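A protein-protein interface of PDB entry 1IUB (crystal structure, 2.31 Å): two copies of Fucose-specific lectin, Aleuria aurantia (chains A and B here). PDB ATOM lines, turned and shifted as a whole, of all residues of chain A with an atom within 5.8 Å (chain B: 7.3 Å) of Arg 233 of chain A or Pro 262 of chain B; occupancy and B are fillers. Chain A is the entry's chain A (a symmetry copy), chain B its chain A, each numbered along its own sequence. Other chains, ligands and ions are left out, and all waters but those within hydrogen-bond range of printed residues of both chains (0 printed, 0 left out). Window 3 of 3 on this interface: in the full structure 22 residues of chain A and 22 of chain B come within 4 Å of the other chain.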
ATOM      1  N   GLN A 230     -31.737  11.356  -7.895  1.00  0.00           N
ATOM      2  CA  GLN A 230     -32.074  10.395  -6.874  1.00  0.00           C
ATOM      3  C   GLN A 230     -31.584  10.834  -5.508  1.00  0.00           C
ATOM      4  O   GLN A 230     -30.472  11.357  -5.359  1.00  0.00           O
ATOM      5  CB  GLN A 230     -31.428   9.060  -7.224  1.00  0.00           C
ATOM      6  CG  GLN A 230     -31.952   7.866  -6.448  1.00  0.00           C
ATOM      7  CD  GLN A 230     -31.091   6.660  -6.643  1.00  0.00           C
ATOM      8  OE1 GLN A 230     -29.998   6.555  -6.059  1.00  0.00           O
ATOM      9  NE2 GLN A 230     -31.544   5.746  -7.480  1.00  0.00           N
ATOM     10  N   LYS A 231     -32.441  10.626  -4.521  1.00  0.00           N
ATOM     11  CA  LYS A 231     -32.117  10.881  -3.133  1.00  0.00           C
ATOM     12  C   LYS A 231     -31.896   9.434  -2.660  1.00  0.00           C
ATOM     13  O   LYS A 231     -32.685   8.552  -2.999  1.00  0.00           O
ATOM     14  CB  LYS A 231     -33.314  11.484  -2.428  1.00  0.00           C
ATOM     15  CG  LYS A 231     -33.160  11.626  -0.926  1.00  0.00           C
ATOM     16  CD  LYS A 231     -32.250  12.748  -0.582  1.00  0.00           C
ATOM     17  CE  LYS A 231     -32.477  13.159   0.848  1.00  0.00           C
ATOM     18  NZ  LYS A 231     -31.426  14.135   1.266  1.00  0.00           N
ATOM     19  N   GLY A 232     -30.820   9.182  -1.914  1.00  0.00           N
ATOM     20  CA  GLY A 232     -30.538   7.831  -1.455  1.00  0.00           C
ATOM     21  C   GLY A 232     -31.703   7.225  -0.701  1.00  0.00           C
ATOM     22  O   GLY A 232     -32.316   7.906   0.105  1.00  0.00           O
ATOM     23  N   ARG A 233     -31.992   5.948  -0.944  1.00  0.00           N
ATOM     24  CA  ARG A 233     -33.106   5.255  -0.306  1.00  0.00           C
ATOM     25  C   ARG A 233     -34.473   5.717  -0.810  1.00  0.00           C
ATOM     26  O   ARG A 233     -35.491   5.413  -0.193  1.00  0.00           O
ATOM     27  CB  ARG A 233     -33.052   5.375   1.214  1.00  0.00           C
ATOM     28  CG  ARG A 233     -32.709   4.068   1.904  1.00  0.00           C
ATOM     29  CD  ARG A 233     -33.759   3.019   1.664  1.00  0.00           C
ATOM     30  NE  ARG A 233     -33.489   1.789   2.416  1.00  0.00           N
ATOM     31  CZ  ARG A 233     -32.560   0.886   2.095  1.00  0.00           C
ATOM     32  NH1 ARG A 233     -31.790   1.057   1.023  1.00  0.00           N
ATOM     33  NH2 ARG A 233     -32.404  -0.198   2.848  1.00  0.00           N
ATOM     34  N   GLU A 234     -34.477   6.474  -1.908  1.00  0.00           N
ATOM     35  CA  GLU A 234     -35.703   6.895  -2.574  1.00  0.00           C
ATOM     36  C   GLU A 234     -35.587   6.272  -3.970  1.00  0.00           C
ATOM     37  O   GLU A 234     -34.583   5.617  -4.277  1.00  0.00           O
ATOM     38  CB  GLU A 234     -35.807   8.407  -2.692  1.00  0.00           C
ATOM     39  CG  GLU A 234     -36.529   9.059  -1.545  1.00  0.00           C
ATOM     40  CD  GLU A 234     -36.650  10.577  -1.707  1.00  0.00           C
ATOM     41  OE1 GLU A 234     -36.763  11.070  -2.861  1.00  0.00           O
ATOM     42  OE2 GLU A 234     -36.647  11.279  -0.668  1.00  0.00           O
ATOM     43  N   GLU A 235     -36.594   6.447  -4.816  1.00  0.00           N
ATOM     44  CA  GLU A 235     -36.506   5.857  -6.150  1.00  0.00           C
ATOM     45  C   GLU A 235     -35.892   6.862  -7.143  1.00  0.00           C
ATOM     46  O   GLU A 235     -35.923   8.066  -6.930  1.00  0.00           O
ATOM     47  CB  GLU A 235     -37.893   5.380  -6.625  1.00  0.00           C
ATOM     48  CG  GLU A 235     -38.574   4.348  -5.684  1.00  0.00           C
ATOM     49  CD  GLU A 235     -38.051   2.915  -5.848  1.00  0.00           C
ATOM     50  OE1 GLU A 235     -37.013   2.692  -6.524  1.00  0.00           O
ATOM     51  OE2 GLU A 235     -38.682   1.991  -5.290  1.00  0.00           O
ATOM     52  N   THR A 258     -36.663   0.960  -3.595  1.00  0.00           N
ATOM     53  CA  THR A 258     -35.578   1.846  -3.165  1.00  0.00           C
ATOM     54  C   THR A 258     -34.272   1.086  -2.849  1.00  0.00           C
ATOM     55  O   THR A 258     -33.815   1.073  -1.720  1.00  0.00           O
ATOM     56  CB  THR A 258     -36.036   2.626  -1.899  1.00  0.00           C
ATOM     57  OG1 THR A 258     -36.333   1.694  -0.852  1.00  0.00           O
ATOM     58  CG2 THR A 258     -37.294   3.420  -2.183  1.00  0.00           C
ATOM     59  N   PRO A 259     -33.664   0.463  -3.861  1.00  0.00           N
ATOM     60  CA  PRO A 259     -32.432  -0.303  -3.686  1.00  0.00           C
ATOM     61  C   PRO A 259     -31.160   0.479  -3.324  1.00  0.00           C
ATOM     62  O   PRO A 259     -30.163  -0.122  -2.981  1.00  0.00           O
ATOM     63  CB  PRO A 259     -32.317  -1.072  -5.010  1.00  0.00           C
ATOM     64  CG  PRO A 259     -32.901  -0.100  -6.020  1.00  0.00           C
ATOM     65  CD  PRO A 259     -34.082   0.514  -5.284  1.00  0.00           C
ATOM     66  N   SER A 260     -31.187   1.806  -3.370  1.00  0.00           N
ATOM     67  CA  SER A 260     -29.989   2.549  -3.023  1.00  0.00           C
ATOM     68  C   SER A 260     -29.917   2.855  -1.516  1.00  0.00           C
ATOM     69  O   SER A 260     -30.938   2.980  -0.854  1.00  0.00           O
ATOM     70  CB  SER A 260     -29.915   3.866  -3.821  1.00  0.00           C
ATOM     71  OG  SER A 260     -30.906   4.816  -3.430  1.00  0.00           O
ATOM     72  N   LEU A 261     -28.705   2.997  -0.986  1.00  0.00           N
ATOM     73  CA  LEU A 261     -28.541   3.323   0.417  1.00  0.00           C
ATOM     74  C   LEU A 261     -28.677   4.827   0.609  1.00  0.00           C
ATOM     75  O   LEU A 261     -28.537   5.616  -0.337  1.00  0.00           O
ATOM     76  CB  LEU A 261     -27.163   2.881   0.912  1.00  0.00           C
ATOM     77  CG  LEU A 261     -26.874   1.380   0.890  1.00  0.00           C
ATOM     78  CD1 LEU A 261     -25.417   1.121   1.180  1.00  0.00           C
ATOM     79  CD2 LEU A 261     -27.780   0.687   1.919  1.00  0.00           C
ATOM     80  N   PRO A 262     -28.957   5.247   1.850  1.00  0.00           N
ATOM     81  CA  PRO A 262     -29.097   6.676   2.144  1.00  0.00           C
ATOM     82  C   PRO A 262     -27.818   7.456   1.819  1.00  0.00           C
ATOM     83  O   PRO A 262     -26.723   6.920   1.933  1.00  0.00           O
ATOM     84  CB  PRO A 262     -29.363   6.706   3.654  1.00  0.00           C
ATOM     85  CG  PRO A 262     -29.990   5.369   3.956  1.00  0.00           C
ATOM     86  CD  PRO A 262     -29.310   4.397   3.011  1.00  0.00           C
ATOM     87  N   ASP A 263     -27.966   8.714   1.413  1.00  0.00           N
ATOM     88  CA  ASP A 263     -26.824   9.610   1.166  1.00  0.00           C
ATOM     89  C   ASP A 263     -25.794   9.207   0.097  1.00  0.00           C
ATOM     90  O   ASP A 263     -24.654   9.684   0.111  1.00  0.00           O
ATOM     91  CB  ASP A 263     -26.094   9.829   2.496  1.00  0.00           C
ATOM     92  CG  ASP A 263     -27.045  10.258   3.618  1.00  0.00           C
ATOM     93  OD1 ASP A 263     -27.028   9.652   4.703  1.00  0.00           O
ATOM     94  OD2 ASP A 263     -27.805  11.206   3.414  1.00  0.00           O
ATOM     95  N   THR A 264     -26.199   8.343  -0.826  1.00  0.00           N
ATOM     96  CA  THR A 264     -25.307   7.900  -1.866  1.00  0.00           C
ATOM     97  C   THR A 264     -25.502   8.749  -3.138  1.00  0.00           C
ATOM     98  O   THR A 264     -26.318   9.652  -3.152  1.00  0.00           O
ATOM     99  CB  THR A 264     -25.534   6.427  -2.153  1.00  0.00           C
ATOM    100  OG1 THR A 264     -26.905   6.237  -2.516  1.00  0.00           O
ATOM    101  CG2 THR A 264     -25.213   5.588  -0.900  1.00  0.00           C
ATOM    102  N   TYR B   6     -18.359   2.331   7.778  1.00  0.00           N
ATOM    103  CA  TYR B   6     -19.755   1.947   7.651  1.00  0.00           C
ATOM    104  C   TYR B   6     -19.883   0.418   7.793  1.00  0.00           C
ATOM    105  O   TYR B   6     -19.226  -0.359   7.094  1.00  0.00           O
ATOM    106  CB  TYR B   6     -20.321   2.445   6.295  1.00  0.00           C
ATOM    107  CG  TYR B   6     -21.714   1.939   5.975  1.00  0.00           C
ATOM    108  CD1 TYR B   6     -22.792   2.206   6.824  1.00  0.00           C
ATOM    109  CD2 TYR B   6     -21.945   1.171   4.832  1.00  0.00           C
ATOM    110  CE1 TYR B   6     -24.071   1.711   6.537  1.00  0.00           C
ATOM    111  CE2 TYR B   6     -23.221   0.686   4.528  1.00  0.00           C
ATOM    112  CZ  TYR B   6     -24.279   0.956   5.391  1.00  0.00           C
ATOM    113  OH  TYR B   6     -25.522   0.445   5.119  1.00  0.00           O
ATOM    114  N   THR B   7     -20.754   0.024   8.718  1.00  0.00           N
ATOM    115  CA  THR B   7     -21.044  -1.352   9.121  1.00  0.00           C
ATOM    116  C   THR B   7     -19.912  -1.913  10.006  1.00  0.00           C
ATOM    117  O   THR B   7     -19.661  -3.112  10.036  1.00  0.00           O
ATOM    118  CB  THR B   7     -21.326  -2.344   7.960  1.00  0.00           C
ATOM    119  OG1 THR B   7     -20.140  -2.598   7.208  1.00  0.00           O
ATOM    120  CG2 THR B   7     -22.426  -1.815   7.050  1.00  0.00           C
ATOM    121  N   LYS B 231     -32.471  -4.275  13.753  1.00  0.00           N
ATOM    122  CA  LYS B 231     -32.174  -4.537  12.361  1.00  0.00           C
ATOM    123  C   LYS B 231     -31.927  -3.094  11.884  1.00  0.00           C
ATOM    124  O   LYS B 231     -32.690  -2.195  12.235  1.00  0.00           O
ATOM    125  CB  LYS B 231     -33.396  -5.112  11.675  1.00  0.00           C
ATOM    126  CG  LYS B 231     -33.269  -5.257  10.171  1.00  0.00           C
ATOM    127  CD  LYS B 231     -32.390  -6.400   9.812  1.00  0.00           C
ATOM    128  CE  LYS B 231     -32.648  -6.805   8.386  1.00  0.00           C
ATOM    129  NZ  LYS B 231     -31.627  -7.805   7.952  1.00  0.00           N
ATOM    130  N   GLY B 232     -30.857  -2.868  11.122  1.00  0.00           N
ATOM    131  CA  GLY B 232     -30.552  -1.523  10.658  1.00  0.00           C
ATOM    132  C   GLY B 232     -31.714  -0.889   9.922  1.00  0.00           C
ATOM    133  O   GLY B 232     -32.355  -1.557   9.126  1.00  0.00           O
ATOM    134  N   ARG B 233     -31.969   0.394  10.169  1.00  0.00           N
ATOM    135  CA  ARG B 233     -33.077   1.112   9.549  1.00  0.00           C
ATOM    136  C   ARG B 233     -34.447   0.682  10.074  1.00  0.00           C
ATOM    137  O   ARG B 233     -35.467   1.009   9.472  1.00  0.00           O
ATOM    138  CB  ARG B 233     -33.050   0.991   8.027  1.00  0.00           C
ATOM    139  CG  ARG B 233     -32.688   2.290   7.332  1.00  0.00           C
ATOM    140  CD  ARG B 233     -33.709   3.362   7.588  1.00  0.00           C
ATOM    141  NE  ARG B 233     -33.423   4.585   6.832  1.00  0.00           N
ATOM    142  CZ  ARG B 233     -32.469   5.467   7.139  1.00  0.00           C
ATOM    143  NH1 ARG B 233     -31.685   5.279   8.198  1.00  0.00           N
ATOM    144  NH2 ARG B 233     -32.299   6.548   6.382  1.00  0.00           N
ATOM    145  N   GLU B 234     -34.451  -0.077  11.172  1.00  0.00           N
ATOM    146  CA  GLU B 234     -35.676  -0.469  11.857  1.00  0.00           C
ATOM    147  C   GLU B 234     -35.524   0.152  13.250  1.00  0.00           C
ATOM    148  O   GLU B 234     -34.501   0.782  13.542  1.00  0.00           O
ATOM    149  CB  GLU B 234     -35.813  -1.977  11.976  1.00  0.00           C
ATOM    150  CG  GLU B 234     -36.567  -2.613  10.841  1.00  0.00           C
ATOM    151  CD  GLU B 234     -36.720  -4.127  11.004  1.00  0.00           C
ATOM    152  OE1 GLU B 234     -36.827  -4.618  12.161  1.00  0.00           O
ATOM    153  OE2 GLU B 234     -36.751  -4.830   9.966  1.00  0.00           O
ATOM    154  N   SER B 260     -31.032   4.515  12.582  1.00  0.00           N
ATOM    155  CA  SER B 260     -29.857   3.745  12.217  1.00  0.00           C
ATOM    156  C   SER B 260     -29.816   3.437  10.708  1.00  0.00           C
ATOM    157  O   SER B 260     -30.849   3.335  10.063  1.00  0.00           O
ATOM    158  CB  SER B 260     -29.801   2.427  13.013  1.00  0.00           C
ATOM    159  OG  SER B 260     -30.819   1.500  12.638  1.00  0.00           O
ATOM    160  N   LEU B 261     -28.616   3.268  10.160  1.00  0.00           N
ATOM    161  CA  LEU B 261     -28.481   2.938   8.755  1.00  0.00           C
ATOM    162  C   LEU B 261     -28.654   1.438   8.564  1.00  0.00           C
ATOM    163  O   LEU B 261     -28.518   0.645   9.509  1.00  0.00           O
ATOM    164  CB  LEU B 261     -27.101   3.348   8.238  1.00  0.00           C
ATOM    165  CG  LEU B 261     -26.778   4.843   8.255  1.00  0.00           C
ATOM    166  CD1 LEU B 261     -25.319   5.068   7.943  1.00  0.00           C
ATOM    167  CD2 LEU B 261     -27.683   5.556   7.240  1.00  0.00           C
ATOM    168  N   PRO B 262     -28.963   1.025   7.328  1.00  0.00           N
ATOM    169  CA  PRO B 262     -29.140  -0.400   7.036  1.00  0.00           C
ATOM    170  C   PRO B 262     -27.875  -1.210   7.342  1.00  0.00           C
ATOM    171  O   PRO B 262     -26.769  -0.699   7.211  1.00  0.00           O
ATOM    172  CB  PRO B 262     -29.430  -0.425   5.531  1.00  0.00           C
ATOM    173  CG  PRO B 262     -30.031   0.927   5.238  1.00  0.00           C
ATOM    174  CD  PRO B 262     -29.315   1.882   6.173  1.00  0.00           C
ATOM    175  N   ASP B 263     -28.046  -2.465   7.751  1.00  0.00           N
ATOM    176  CA  ASP B 263     -26.920  -3.386   7.980  1.00  0.00           C
ATOM    177  C   ASP B 263     -25.866  -3.008   9.033  1.00  0.00           C
ATOM    178  O   ASP B 263     -24.737  -3.511   9.001  1.00  0.00           O
ATOM    179  CB  ASP B 263     -26.216  -3.622   6.640  1.00  0.00           C
ATOM    180  CG  ASP B 263     -27.195  -4.028   5.531  1.00  0.00           C
ATOM    181  OD1 ASP B 263     -27.180  -3.423   4.447  1.00  0.00           O
ATOM    182  OD2 ASP B 263     -27.973  -4.960   5.748  1.00  0.00           O
ATOM    183  N   THR B 264     -26.237  -2.135   9.962  1.00  0.00           N
ATOM    184  CA  THR B 264     -25.318  -1.713  10.988  1.00  0.00           C
ATOM    185  C   THR B 264     -25.513  -2.557  12.263  1.00  0.00           C
ATOM    186  O   THR B 264     -26.350  -3.441  12.290  1.00  0.00           O
ATOM    187  CB  THR B 264     -25.506  -0.235  11.278  1.00  0.00           C
ATOM    188  OG1 THR B 264     -26.867  -0.014  11.662  1.00  0.00           O
ATOM    189  CG2 THR B 264     -25.186   0.597  10.020  1.00  0.00           C
ATOM    190  N   PHE B 265     -24.713  -2.286  13.290  1.00  0.00           N
ATOM    191  CA  PHE B 265     -24.747  -3.055  14.510  1.00  0.00           C
ATOM    192  C   PHE B 265     -24.900  -2.153  15.713  1.00  0.00           C
ATOM    193  O   PHE B 265     -24.810  -0.920  15.596  1.00  0.00           O
ATOM    194  CB  PHE B 265     -23.451  -3.872  14.645  1.00  0.00           C
ATOM    195  CG  PHE B 265     -23.175  -4.761  13.476  1.00  0.00           C
ATOM    196  CD1 PHE B 265     -22.411  -4.303  12.396  1.00  0.00           C
ATOM    197  CD2 PHE B 265     -23.752  -6.013  13.399  1.00  0.00           C
ATOM    198  CE1 PHE B 265     -22.239  -5.095  11.240  1.00  0.00           C
ATOM    199  CE2 PHE B 265     -23.597  -6.823  12.249  1.00  0.00           C
ATOM    200  CZ  PHE B 265     -22.842  -6.362  11.166  1.00  0.00           C
ATOM    201  N   GLN B 281     -25.120   3.081  14.636  1.00  0.00           N
ATOM    202  CA  GLN B 281     -24.459   3.846  13.578  1.00  0.00           C
ATOM    203  C   GLN B 281     -25.525   4.529  12.717  1.00  0.00           C
ATOM    204  O   GLN B 281     -26.414   3.875  12.158  1.00  0.00           O
ATOM    205  CB  GLN B 281     -23.596   2.901  12.730  1.00  0.00           C
ATOM    206  CG  GLN B 281     -22.746   3.622  11.701  1.00  0.00           C
ATOM    207  CD  GLN B 281     -21.693   2.729  11.064  1.00  0.00           C
ATOM    208  OE1 GLN B 281     -22.014   1.718  10.427  1.00  0.00           O
ATOM    209  NE2 GLN B 281     -20.429   3.103  11.225  1.00  0.00           N
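OH of Tyr 6 of chain B is in hydrogen-bond range of O of Pro 262 of chain B, at 2.7 Å.
The guanidinium group (NH1) of Arg 233 of chain B sits at hydrogen-bond distance from the backbone carbonyl oxygen (O) of Ser 260 of chain B (2.8 Å).
NH1 of Arg 233 of chain A lies within hydrogen-bond range of O of Thr 258 of chain A (3.4 Å).
The guanidinium group (NH1) of Arg 233 of chain A is in hydrogen-bond range of the backbone carbonyl oxygen (O) of Ser 260 of chain A, 2.8 Å away.
The side-chain hydroxyl of Thr 264 of chain A sits at hydrogen-bond distance from the backbone carbonyl oxygen of Leu 261 of chain A.
Of the printed residues of chain B, Arg 233 of chain A touches Pro 262 (3.6 Å).
Of the printed residues of chain A, Pro 262 of chain B touches Arg 233.
Of the printed residues of chain A, Tyr 6 of chain B touches Leu 261.
Of the printed residues of chain B, Pro 262 of chain A touches Arg 233 (3.6 Å).
Of the printed residues of chain A, Arg 233 of chain B touches Pro 262.
Printed residues of chain B within 4 Å of Leu 261 of chain A: Tyr 6.
Gln 230 of chain A touches none of the printed residues of chain B.
The nearest residue of chain B that does not touch Arg 233 of chain A is Arg 233 of chain B (5.0 Å).
Among the printed residues, merely in contact across the chains: Pro 262 of chain A with Arg 233 of chain B, Arg 233 of chain A with Pro 262 of chain B and Leu 261 of chain A with Tyr 6 of chain B.
Arg 233 of chain A touches Pro 262 of chain B, and with the chains exchanged Pro 262 of chain A touches Arg 233 of chain B.
Positions printed for both chains: 231, 232, 233, 234, 260, 261, 262, 263 and 264.
Of the 13 printed residues of chain A, 3 touch a printed residue of chain B.
Hydrophobic or aromatic side chains of chain A within 4 Å of the printed part of chain B: Leu 261 and Pro 262.
Of the 13 printed residues of chain B, 3 touch a printed residue of chain A.
Hydrophobic or aromatic side chains of chain B within 4 Å of the printed part of chain A: Tyr 6 and Pro 262.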
